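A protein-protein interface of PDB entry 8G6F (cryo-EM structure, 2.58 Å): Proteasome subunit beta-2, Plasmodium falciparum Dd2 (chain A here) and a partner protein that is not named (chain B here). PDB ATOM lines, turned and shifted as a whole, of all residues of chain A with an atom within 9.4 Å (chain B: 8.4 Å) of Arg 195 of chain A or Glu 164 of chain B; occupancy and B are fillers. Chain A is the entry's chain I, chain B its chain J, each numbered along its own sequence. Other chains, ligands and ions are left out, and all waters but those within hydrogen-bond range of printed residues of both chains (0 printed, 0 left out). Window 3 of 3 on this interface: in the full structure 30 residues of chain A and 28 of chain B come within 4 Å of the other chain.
OE2 of Glu 164 of chain B is in salt-bridge range of NZ of Lys 29 of chain A (3.1 Å).
NE of Arg 195 of chain A sits at hydrogen-bond distance from O of Tyr 197 of chain A (2.8 Å).
Ile 25 of chain A touches Glu 157 of chain B (CD1 to OE1, 3.5 Å).
Arg 195 of chain A touches Glu 164 of chain B.
Of the printed residues of chain B, Ile 25 of chain A touches Glu 157 (3.5 Å).
Printed residues of chain B within 4 Å of Lys 29 of chain A: Glu 164.
Of chain B, only Glu 164 (3.8 Å) comes within 4 Å of Arg 195 of chain A.
Val 151 of chain B touches none of the printed residues of chain A.
No residue of chain A comes within 4 Å of Gly 161 of chain B.
No residue of chain A comes within 4 Å of Cys 163 of chain B.
Glu 164 of chain B touches just these residues of chain A: Lys 29 (3.1 Å) and Arg 195 (3.8 Å).
The nearest residue of chain B that does not touch Arg 195 of chain A is Ser 165 of chain B (5.1 Å).
Hydrophobic or aromatic side chains of chain A that line the printed part of chain B: Ile 25.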
ATOM      1  N   ILE A  25     -26.668 -12.696 -17.604  1.00  0.00           N
ATOM      2  CA  ILE A  25     -25.840 -11.502 -17.495  1.00  0.00           C
ATOM      3  C   ILE A  25     -24.474 -11.790 -18.096  1.00  0.00           C
ATOM      4  O   ILE A  25     -23.891 -12.852 -17.858  1.00  0.00           O
ATOM      5  CB  ILE A  25     -25.705 -11.045 -16.030  1.00  0.00           C
ATOM      6  CG1 ILE A  25     -27.079 -10.730 -15.436  1.00  0.00           C
ATOM      7  CG2 ILE A  25     -24.790  -9.842 -15.935  1.00  0.00           C
ATOM      8  CD1 ILE A  25     -27.798  -9.574 -16.098  1.00  0.00           C
ATOM      9  N   VAL A  26     -23.967 -10.838 -18.870  1.00  0.00           N
ATOM     10  CA  VAL A  26     -22.647 -10.957 -19.478  1.00  0.00           C
ATOM     11  C   VAL A  26     -21.609 -10.611 -18.417  1.00  0.00           C
ATOM     12  O   VAL A  26     -21.476  -9.452 -18.019  1.00  0.00           O
ATOM     13  CB  VAL A  26     -22.514 -10.051 -20.706  1.00  0.00           C
ATOM     14  CG1 VAL A  26     -21.141 -10.184 -21.322  1.00  0.00           C
ATOM     15  CG2 VAL A  26     -23.586 -10.389 -21.718  1.00  0.00           C
ATOM     16  N   ALA A  27     -20.876 -11.621 -17.947  1.00  0.00           N
ATOM     17  CA  ALA A  27     -19.845 -11.394 -16.944  1.00  0.00           C
ATOM     18  C   ALA A  27     -18.554 -10.875 -17.557  1.00  0.00           C
ATOM     19  O   ALA A  27     -17.806 -10.150 -16.893  1.00  0.00           O
ATOM     20  CB  ALA A  27     -19.570 -12.685 -16.175  1.00  0.00           C
ATOM     21  N   ASP A  28     -18.276 -11.232 -18.808  1.00  0.00           N
ATOM     22  CA  ASP A  28     -17.067 -10.797 -19.491  1.00  0.00           C
ATOM     23  C   ASP A  28     -17.405 -10.569 -20.954  1.00  0.00           C
ATOM     24  O   ASP A  28     -17.986 -11.444 -21.597  1.00  0.00           O
ATOM     25  CB  ASP A  28     -15.952 -11.838 -19.357  1.00  0.00           C
ATOM     26  CG  ASP A  28     -14.586 -11.287 -19.698  1.00  0.00           C
ATOM     27  OD1 ASP A  28     -14.494 -10.107 -20.093  1.00  0.00           O
ATOM     28  OD2 ASP A  28     -13.599 -12.040 -19.573  1.00  0.00           O
ATOM     29  N   LYS A  29     -17.042  -9.397 -21.470  1.00  0.00           N
ATOM     30  CA  LYS A  29     -17.326  -9.054 -22.855  1.00  0.00           C
ATOM     31  C   LYS A  29     -16.207  -9.438 -23.808  1.00  0.00           C
ATOM     32  O   LYS A  29     -16.456  -9.558 -25.012  1.00  0.00           O
ATOM     33  CB  LYS A  29     -17.579  -7.553 -22.990  1.00  0.00           C
ATOM     34  CG  LYS A  29     -18.820  -7.060 -22.294  1.00  0.00           C
ATOM     35  CD  LYS A  29     -18.740  -5.568 -22.040  1.00  0.00           C
ATOM     36  CE  LYS A  29     -20.006  -4.864 -22.464  1.00  0.00           C
ATOM     37  NZ  LYS A  29     -19.805  -3.397 -22.554  1.00  0.00           N
ATOM     38  N   ASN A 172     -16.254 -10.133 -29.906  1.00  0.00           N
ATOM     39  CA  ASN A 172     -15.474 -10.108 -31.128  1.00  0.00           C
ATOM     40  C   ASN A 172     -15.231 -11.529 -31.622  1.00  0.00           C
ATOM     41  O   ASN A 172     -15.630 -12.513 -30.998  1.00  0.00           O
ATOM     42  CB  ASN A 172     -14.150  -9.379 -30.900  1.00  0.00           C
ATOM     43  CG  ASN A 172     -14.328  -8.067 -30.178  1.00  0.00           C
ATOM     44  OD1 ASN A 172     -15.117  -7.225 -30.589  1.00  0.00           O
ATOM     45  ND2 ASN A 172     -13.590  -7.884 -29.094  1.00  0.00           N
ATOM     46  N   GLU A 191     -14.354  -7.668 -34.597  1.00  0.00           N
ATOM     47  CA  GLU A 191     -14.933  -6.564 -33.832  1.00  0.00           C
ATOM     48  C   GLU A 191     -16.269  -6.120 -34.418  1.00  0.00           C
ATOM     49  O   GLU A 191     -16.406  -4.961 -34.825  1.00  0.00           O
ATOM     50  CB  GLU A 191     -13.977  -5.372 -33.788  1.00  0.00           C
ATOM     51  CG  GLU A 191     -12.747  -5.586 -32.935  1.00  0.00           C
ATOM     52  CD  GLU A 191     -12.556  -4.490 -31.909  1.00  0.00           C
ATOM     53  OE1 GLU A 191     -13.530  -4.162 -31.203  1.00  0.00           O
ATOM     54  OE2 GLU A 191     -11.434  -3.953 -31.811  1.00  0.00           O
ATOM     55  N   PRO A 192     -17.281  -6.990 -34.468  1.00  0.00           N
ATOM     56  CA  PRO A 192     -18.540  -6.631 -35.128  1.00  0.00           C
ATOM     57  C   PRO A 192     -19.583  -5.966 -34.244  1.00  0.00           C
ATOM     58  O   PRO A 192     -20.588  -5.479 -34.777  1.00  0.00           O
ATOM     59  CB  PRO A 192     -19.045  -7.992 -35.621  1.00  0.00           C
ATOM     60  CG  PRO A 192     -18.559  -8.954 -34.598  1.00  0.00           C
ATOM     61  CD  PRO A 192     -17.302  -8.383 -33.989  1.00  0.00           C
ATOM     62  N   ASN A 193     -19.388  -5.930 -32.929  1.00  0.00           N
ATOM     63  CA  ASN A 193     -20.362  -5.375 -32.000  1.00  0.00           C
ATOM     64  C   ASN A 193     -19.729  -4.242 -31.210  1.00  0.00           C
ATOM     65  O   ASN A 193     -18.668  -4.419 -30.607  1.00  0.00           O
ATOM     66  CB  ASN A 193     -20.882  -6.444 -31.040  1.00  0.00           C
ATOM     67  CG  ASN A 193     -21.601  -7.559 -31.753  1.00  0.00           C
ATOM     68  OD1 ASN A 193     -21.068  -8.655 -31.914  1.00  0.00           O
ATOM     69  ND2 ASN A 193     -22.821  -7.285 -32.191  1.00  0.00           N
ATOM     70  N   MET A 194     -20.388  -3.088 -31.215  1.00  0.00           N
ATOM     71  CA  MET A 194     -19.967  -1.941 -30.429  1.00  0.00           C
ATOM     72  C   MET A 194     -21.205  -1.204 -29.947  1.00  0.00           C
ATOM     73  O   MET A 194     -22.255  -1.240 -30.592  1.00  0.00           O
ATOM     74  CB  MET A 194     -19.074  -0.995 -31.240  1.00  0.00           C
ATOM     75  CG  MET A 194     -19.708  -0.499 -32.529  1.00  0.00           C
ATOM     76  SD  MET A 194     -18.792   0.854 -33.286  1.00  0.00           S
ATOM     77  CE  MET A 194     -18.723   0.306 -34.991  1.00  0.00           C
ATOM     78  N   ARG A 195     -21.075  -0.539 -28.804  1.00  0.00           N
ATOM     79  CA  ARG A 195     -22.171   0.267 -28.290  1.00  0.00           C
ATOM     80  C   ARG A 195     -22.545   1.335 -29.309  1.00  0.00           C
ATOM     81  O   ARG A 195     -21.680   2.049 -29.823  1.00  0.00           O
ATOM     82  CB  ARG A 195     -21.768   0.896 -26.959  1.00  0.00           C
ATOM     83  CG  ARG A 195     -22.665   2.013 -26.506  1.00  0.00           C
ATOM     84  CD  ARG A 195     -22.496   2.292 -25.034  1.00  0.00           C
ATOM     85  NE  ARG A 195     -23.509   3.223 -24.555  1.00  0.00           N
ATOM     86  CZ  ARG A 195     -24.068   3.183 -23.354  1.00  0.00           C
ATOM     87  NH1 ARG A 195     -23.726   2.272 -22.459  1.00  0.00           N
ATOM     88  NH2 ARG A 195     -24.994   4.085 -23.042  1.00  0.00           N
ATOM     89  N   LEU A 196     -23.840   1.444 -29.602  1.00  0.00           N
ATOM     90  CA  LEU A 196     -24.306   2.232 -30.735  1.00  0.00           C
ATOM     91  C   LEU A 196     -24.760   3.637 -30.372  1.00  0.00           C
ATOM     92  O   LEU A 196     -24.775   4.506 -31.250  1.00  0.00           O
ATOM     93  CB  LEU A 196     -25.462   1.512 -31.441  1.00  0.00           C
ATOM     94  CG  LEU A 196     -25.113   0.314 -32.325  1.00  0.00           C
ATOM     95  CD1 LEU A 196     -26.344  -0.155 -33.066  1.00  0.00           C
ATOM     96  CD2 LEU A 196     -24.002   0.644 -33.307  1.00  0.00           C
ATOM     97  N   TYR A 197     -25.138   3.888 -29.123  1.00  0.00           N
ATOM     98  CA  TYR A 197     -25.561   5.213 -28.693  1.00  0.00           C
ATOM     99  C   TYR A 197     -24.669   5.689 -27.558  1.00  0.00           C
ATOM    100  O   TYR A 197     -24.386   4.933 -26.626  1.00  0.00           O
ATOM    101  CB  TYR A 197     -27.021   5.223 -28.240  1.00  0.00           C
ATOM    102  CG  TYR A 197     -27.437   6.553 -27.662  1.00  0.00           C
ATOM    103  CD1 TYR A 197     -27.793   7.608 -28.488  1.00  0.00           C
ATOM    104  CD2 TYR A 197     -27.449   6.764 -26.291  1.00  0.00           C
ATOM    105  CE1 TYR A 197     -28.159   8.824 -27.966  1.00  0.00           C
ATOM    106  CE2 TYR A 197     -27.812   7.977 -25.763  1.00  0.00           C
ATOM    107  CZ  TYR A 197     -28.169   9.003 -26.605  1.00  0.00           C
ATOM    108  OH  TYR A 197     -28.532  10.215 -26.079  1.00  0.00           O
ATOM    109  N   HIS A 198     -24.241   6.944 -27.641  1.00  0.00           N
ATOM    110  CA  HIS A 198     -23.473   7.585 -26.587  1.00  0.00           C
ATOM    111  C   HIS A 198     -24.092   8.940 -26.284  1.00  0.00           C
ATOM    112  O   HIS A 198     -24.617   9.611 -27.174  1.00  0.00           O
ATOM    113  CB  HIS A 198     -22.002   7.753 -26.987  1.00  0.00           C
ATOM    114  CG  HIS A 198     -21.246   6.464 -27.053  1.00  0.00           C
ATOM    115  ND1 HIS A 198     -21.211   5.680 -28.185  1.00  0.00           N
ATOM    116  CD2 HIS A 198     -20.502   5.819 -26.126  1.00  0.00           C
ATOM    117  CE1 HIS A 198     -20.477   4.607 -27.952  1.00  0.00           C
ATOM    118  NE2 HIS A 198     -20.037   4.666 -26.709  1.00  0.00           N
ATOM    119  N   LEU A 199     -24.034   9.332 -25.017  1.00  0.00           N
ATOM    120  CA  LEU A 199     -24.574  10.619 -24.627  1.00  0.00           C
ATOM    121  C   LEU A 199     -23.739  11.740 -25.243  1.00  0.00           C
ATOM    122  O   LEU A 199     -22.561  11.548 -25.553  1.00  0.00           O
ATOM    123  CB  LEU A 199     -24.591  10.758 -23.108  1.00  0.00           C
ATOM    124  CG  LEU A 199     -25.776  10.120 -22.380  1.00  0.00           C
ATOM    125  CD1 LEU A 199     -25.558  10.148 -20.879  1.00  0.00           C
ATOM    126  CD2 LEU A 199     -27.072  10.817 -22.734  1.00  0.00           C
ATOM    127  N   PRO A 200     -24.329  12.920 -25.445  1.00  0.00           N
ATOM    128  CA  PRO A 200     -23.547  14.020 -26.032  1.00  0.00           C
ATOM    129  C   PRO A 200     -22.277  14.339 -25.264  1.00  0.00           C
ATOM    130  O   PRO A 200     -21.248  14.635 -25.883  1.00  0.00           O
ATOM    131  CB  PRO A 200     -24.539  15.187 -26.018  1.00  0.00           C
ATOM    132  CG  PRO A 200     -25.866  14.544 -26.098  1.00  0.00           C
ATOM    133  CD  PRO A 200     -25.756  13.264 -25.329  1.00  0.00           C
ATOM    134  N   LEU B  13     -16.603  -3.550  -5.544  1.00  0.00           N
ATOM    135  CA  LEU B  13     -16.490  -2.857  -6.814  1.00  0.00           C
ATOM    136  C   LEU B  13     -15.063  -2.349  -6.964  1.00  0.00           C
ATOM    137  O   LEU B  13     -14.399  -2.037  -5.978  1.00  0.00           O
ATOM    138  CB  LEU B  13     -17.502  -1.704  -6.884  1.00  0.00           C
ATOM    139  CG  LEU B  13     -17.390  -0.659  -7.990  1.00  0.00           C
ATOM    140  CD1 LEU B  13     -17.624  -1.269  -9.349  1.00  0.00           C
ATOM    141  CD2 LEU B  13     -18.377   0.451  -7.737  1.00  0.00           C
ATOM    142  N   MET B  15     -12.483   0.084  -9.775  1.00  0.00           N
ATOM    143  CA  MET B  15     -12.458   0.981 -10.918  1.00  0.00           C
ATOM    144  C   MET B  15     -11.037   1.475 -11.130  1.00  0.00           C
ATOM    145  O   MET B  15     -10.237   1.510 -10.199  1.00  0.00           O
ATOM    146  CB  MET B  15     -13.405   2.167 -10.710  1.00  0.00           C
ATOM    147  CG  MET B  15     -14.247   2.511 -11.912  1.00  0.00           C
ATOM    148  SD  MET B  15     -15.396   3.856 -11.591  1.00  0.00           S
ATOM    149  CE  MET B  15     -16.955   3.054 -11.936  1.00  0.00           C
ATOM    150  N   ASP B 148     -11.303  -1.244 -17.089  1.00  0.00           N
ATOM    151  CA  ASP B 148     -12.114  -0.135 -16.604  1.00  0.00           C
ATOM    152  C   ASP B 148     -12.728  -0.407 -15.236  1.00  0.00           C
ATOM    153  O   ASP B 148     -12.492   0.358 -14.301  1.00  0.00           O
ATOM    154  CB  ASP B 148     -13.212   0.208 -17.623  1.00  0.00           C
ATOM    155  CG  ASP B 148     -13.820  -1.009 -18.271  1.00  0.00           C
ATOM    156  OD1 ASP B 148     -13.631  -2.119 -17.751  1.00  0.00           O
ATOM    157  OD2 ASP B 148     -14.494  -0.856 -19.307  1.00  0.00           O
ATOM    158  N   PHE B 149     -13.504  -1.477 -15.080  1.00  0.00           N
ATOM    159  CA  PHE B 149     -14.174  -1.712 -13.811  1.00  0.00           C
ATOM    160  C   PHE B 149     -14.519  -3.187 -13.671  1.00  0.00           C
ATOM    161  O   PHE B 149     -14.777  -3.875 -14.657  1.00  0.00           O
ATOM    162  CB  PHE B 149     -15.441  -0.857 -13.686  1.00  0.00           C
ATOM    163  CG  PHE B 149     -16.397  -1.026 -14.827  1.00  0.00           C
ATOM    164  CD1 PHE B 149     -17.311  -2.062 -14.836  1.00  0.00           C
ATOM    165  CD2 PHE B 149     -16.377  -0.155 -15.896  1.00  0.00           C
ATOM    166  CE1 PHE B 149     -18.183  -2.221 -15.886  1.00  0.00           C
ATOM    167  CE2 PHE B 149     -17.246  -0.313 -16.946  1.00  0.00           C
ATOM    168  CZ  PHE B 149     -18.149  -1.346 -16.940  1.00  0.00           C
ATOM    169  N   VAL B 151     -16.873  -5.846 -10.914  1.00  0.00           N
ATOM    170  CA  VAL B 151     -17.898  -5.866  -9.882  1.00  0.00           C
ATOM    171  C   VAL B 151     -18.055  -7.293  -9.387  1.00  0.00           C
ATOM    172  O   VAL B 151     -17.699  -8.253 -10.070  1.00  0.00           O
ATOM    173  CB  VAL B 151     -19.253  -5.317 -10.387  1.00  0.00           C
ATOM    174  CG1 VAL B 151     -19.046  -4.074 -11.225  1.00  0.00           C
ATOM    175  CG2 VAL B 151     -20.004  -6.371 -11.179  1.00  0.00           C
ATOM    176  N   GLU B 157     -25.746  -6.888 -10.779  1.00  0.00           N
ATOM    177  CA  GLU B 157     -26.496  -6.316 -11.894  1.00  0.00           C
ATOM    178  C   GLU B 157     -26.587  -4.801 -11.775  1.00  0.00           C
ATOM    179  O   GLU B 157     -26.358  -4.070 -12.748  1.00  0.00           O
ATOM    180  CB  GLU B 157     -27.894  -6.929 -11.956  1.00  0.00           C
ATOM    181  CG  GLU B 157     -27.968  -8.196 -12.779  1.00  0.00           C
ATOM    182  CD  GLU B 157     -29.385  -8.682 -12.971  1.00  0.00           C
ATOM    183  OE1 GLU B 157     -30.090  -8.127 -13.839  1.00  0.00           O
ATOM    184  OE2 GLU B 157     -29.796  -9.618 -12.254  1.00  0.00           O
ATOM    185  N   GLN B 158     -26.927  -4.311 -10.585  1.00  0.00           N
ATOM    186  CA  GLN B 158     -27.000  -2.872 -10.376  1.00  0.00           C
ATOM    187  C   GLN B 158     -25.646  -2.218 -10.605  1.00  0.00           C
ATOM    188  O   GLN B 158     -25.555  -1.157 -11.234  1.00  0.00           O
ATOM    189  CB  GLN B 158     -27.507  -2.580  -8.967  1.00  0.00           C
ATOM    190  CG  GLN B 158     -28.945  -2.990  -8.731  1.00  0.00           C
ATOM    191  CD  GLN B 158     -29.075  -4.365  -8.117  1.00  0.00           C
ATOM    192  OE1 GLN B 158     -28.594  -5.352  -8.664  1.00  0.00           O
ATOM    193  NE2 GLN B 158     -29.732  -4.435  -6.973  1.00  0.00           N
ATOM    194  N   LEU B 159     -24.578  -2.839 -10.102  1.00  0.00           N
ATOM    195  CA  LEU B 159     -23.248  -2.274 -10.294  1.00  0.00           C
ATOM    196  C   LEU B 159     -22.853  -2.276 -11.764  1.00  0.00           C
ATOM    197  O   LEU B 159     -22.248  -1.316 -12.248  1.00  0.00           O
ATOM    198  CB  LEU B 159     -22.233  -3.045  -9.455  1.00  0.00           C
ATOM    199  CG  LEU B 159     -22.281  -2.756  -7.955  1.00  0.00           C
ATOM    200  CD1 LEU B 159     -21.459  -3.770  -7.188  1.00  0.00           C
ATOM    201  CD2 LEU B 159     -21.800  -1.350  -7.668  1.00  0.00           C
ATOM    202  N   PHE B 160     -23.186  -3.343 -12.491  1.00  0.00           N
ATOM    203  CA  PHE B 160     -22.891  -3.397 -13.916  1.00  0.00           C
ATOM    204  C   PHE B 160     -23.607  -2.285 -14.662  1.00  0.00           C
ATOM    205  O   PHE B 160     -23.014  -1.621 -15.515  1.00  0.00           O
ATOM    206  CB  PHE B 160     -23.305  -4.754 -14.488  1.00  0.00           C
ATOM    207  CG  PHE B 160     -22.214  -5.783 -14.484  1.00  0.00           C
ATOM    208  CD1 PHE B 160     -20.942  -5.479 -14.932  1.00  0.00           C
ATOM    209  CD2 PHE B 160     -22.470  -7.066 -14.043  1.00  0.00           C
ATOM    210  CE1 PHE B 160     -19.950  -6.431 -14.928  1.00  0.00           C
ATOM    211  CE2 PHE B 160     -21.479  -8.018 -14.041  1.00  0.00           C
ATOM    212  CZ  PHE B 160     -20.218  -7.699 -14.483  1.00  0.00           C
ATOM    213  N   GLY B 161     -24.884  -2.066 -14.355  1.00  0.00           N
ATOM    214  CA  GLY B 161     -25.606  -0.993 -15.019  1.00  0.00           C
ATOM    215  C   GLY B 161     -25.013   0.368 -14.719  1.00  0.00           C
ATOM    216  O   GLY B 161     -24.781   1.179 -15.623  1.00  0.00           O
ATOM    217  N   MET B 162     -24.736   0.630 -13.440  1.00  0.00           N
ATOM    218  CA  MET B 162     -24.193   1.928 -13.061  1.00  0.00           C
ATOM    219  C   MET B 162     -22.833   2.163 -13.698  1.00  0.00           C
ATOM    220  O   MET B 162     -22.543   3.269 -14.162  1.00  0.00           O
ATOM    221  CB  MET B 162     -24.096   2.029 -11.541  1.00  0.00           C
ATOM    222  CG  MET B 162     -25.417   2.336 -10.854  1.00  0.00           C
ATOM    223  SD  MET B 162     -26.150   3.929 -11.266  1.00  0.00           S
ATOM    224  CE  MET B 162     -24.727   5.001 -11.342  1.00  0.00           C
ATOM    225  N   CYS B 163     -21.982   1.138 -13.731  1.00  0.00           N
ATOM    226  CA  CYS B 163     -20.646   1.303 -14.288  1.00  0.00           C
ATOM    227  C   CYS B 163     -20.675   1.409 -15.804  1.00  0.00           C
ATOM    228  O   CYS B 163     -19.860   2.131 -16.387  1.00  0.00           O
ATOM    229  CB  CYS B 163     -19.758   0.141 -13.855  1.00  0.00           C
ATOM    230  SG  CYS B 163     -19.224   0.216 -12.140  1.00  0.00           S
ATOM    231  N   GLU B 164     -21.588   0.696 -16.464  1.00  0.00           N
ATOM    232  CA  GLU B 164     -21.732   0.855 -17.904  1.00  0.00           C
ATOM    233  C   GLU B 164     -22.176   2.266 -18.249  1.00  0.00           C
ATOM    234  O   GLU B 164     -21.718   2.842 -19.241  1.00  0.00           O
ATOM    235  CB  GLU B 164     -22.732  -0.164 -18.452  1.00  0.00           C
ATOM    236  CG  GLU B 164     -22.186  -1.574 -18.559  1.00  0.00           C
ATOM    237  CD  GLU B 164     -21.049  -1.682 -19.543  1.00  0.00           C
ATOM    238  OE1 GLU B 164     -20.844  -0.726 -20.317  1.00  0.00           O
ATOM    239  OE2 GLU B 164     -20.357  -2.719 -19.545  1.00  0.00           O
ATOM    240  N   SER B 165     -23.071   2.840 -17.445  1.00  0.00           N
ATOM    241  CA  SER B 165     -23.578   4.165 -17.771  1.00  0.00           C
ATOM    242  C   SER B 165     -22.630   5.287 -17.369  1.00  0.00           C
ATOM    243  O   SER B 165     -22.543   6.291 -18.080  1.00  0.00           O
ATOM    244  CB  SER B 165     -24.937   4.376 -17.111  1.00  0.00           C
ATOM    245  OG  SER B 165     -25.975   4.051 -18.015  1.00  0.00           O
ATOM    246  N   LEU B 166     -21.912   5.151 -16.252  1.00  0.00           N
ATOM    247  CA  LEU B 166     -21.245   6.290 -15.639  1.00  0.00           C
ATOM    248  C   LEU B 166     -19.725   6.238 -15.677  1.00  0.00           C
ATOM    249  O   LEU B 166     -19.093   7.271 -15.448  1.00  0.00           O
ATOM    250  CB  LEU B 166     -21.684   6.435 -14.174  1.00  0.00           C
ATOM    251  CG  LEU B 166     -22.923   7.287 -13.874  1.00  0.00           C
ATOM    252  CD1 LEU B 166     -22.776   8.700 -14.409  1.00  0.00           C
ATOM    253  CD2 LEU B 166     -24.177   6.645 -14.429  1.00  0.00           C
ATOM    254  N   TYR B 167     -19.121   5.085 -15.952  1.00  0.00           N
ATOM    255  CA  TYR B 167     -17.666   5.010 -15.964  1.00  0.00           C
ATOM    256  C   TYR B 167     -17.095   5.935 -17.029  1.00  0.00           C
ATOM    257  O   TYR B 167     -17.578   5.970 -18.163  1.00  0.00           O
ATOM    258  CB  TYR B 167     -17.198   3.579 -16.212  1.00  0.00           C
ATOM    259  CG  TYR B 167     -15.712   3.490 -16.479  1.00  0.00           C
ATOM    260  CD1 TYR B 167     -14.799   3.468 -15.435  1.00  0.00           C
ATOM    261  CD2 TYR B 167     -15.224   3.449 -17.774  1.00  0.00           C
ATOM    262  CE1 TYR B 167     -13.449   3.399 -15.675  1.00  0.00           C
ATOM    263  CE2 TYR B 167     -13.872   3.381 -18.021  1.00  0.00           C
ATOM    264  CZ  TYR B 167     -12.991   3.359 -16.970  1.00  0.00           C
ATOM    265  OH  TYR B 167     -11.643   3.291 -17.217  1.00  0.00           O
ATOM    266  N   VAL B 168     -16.058   6.681 -16.661  1.00  0.00           N
ATOM    267  CA  VAL B 168     -15.357   7.585 -17.563  1.00  0.00           C
ATOM    268  C   VAL B 168     -13.882   7.218 -17.546  1.00  0.00           C
ATOM    269  O   VAL B 168     -13.278   7.103 -16.474  1.00  0.00           O
ATOM    270  CB  VAL B 168     -15.558   9.059 -17.167  1.00  0.00           C
ATOM    271  CG1 VAL B 168     -14.778   9.968 -18.093  1.00  0.00           C
ATOM    272  CG2 VAL B 168     -17.029   9.420 -17.185  1.00  0.00           C
ATOM    273  N   CYS B 183     -21.464   5.229  -8.166  1.00  0.00           N
ATOM    274  CA  CYS B 183     -21.892   3.923  -8.648  1.00  0.00           C
ATOM    275  C   CYS B 183     -22.276   3.018  -7.486  1.00  0.00           C
ATOM    276  O   CYS B 183     -23.349   2.404  -7.489  1.00  0.00           O
ATOM    277  CB  CYS B 183     -20.777   3.285  -9.479  1.00  0.00           C
ATOM    278  SG  CYS B 183     -20.492   4.056 -11.083  1.00  0.00           S
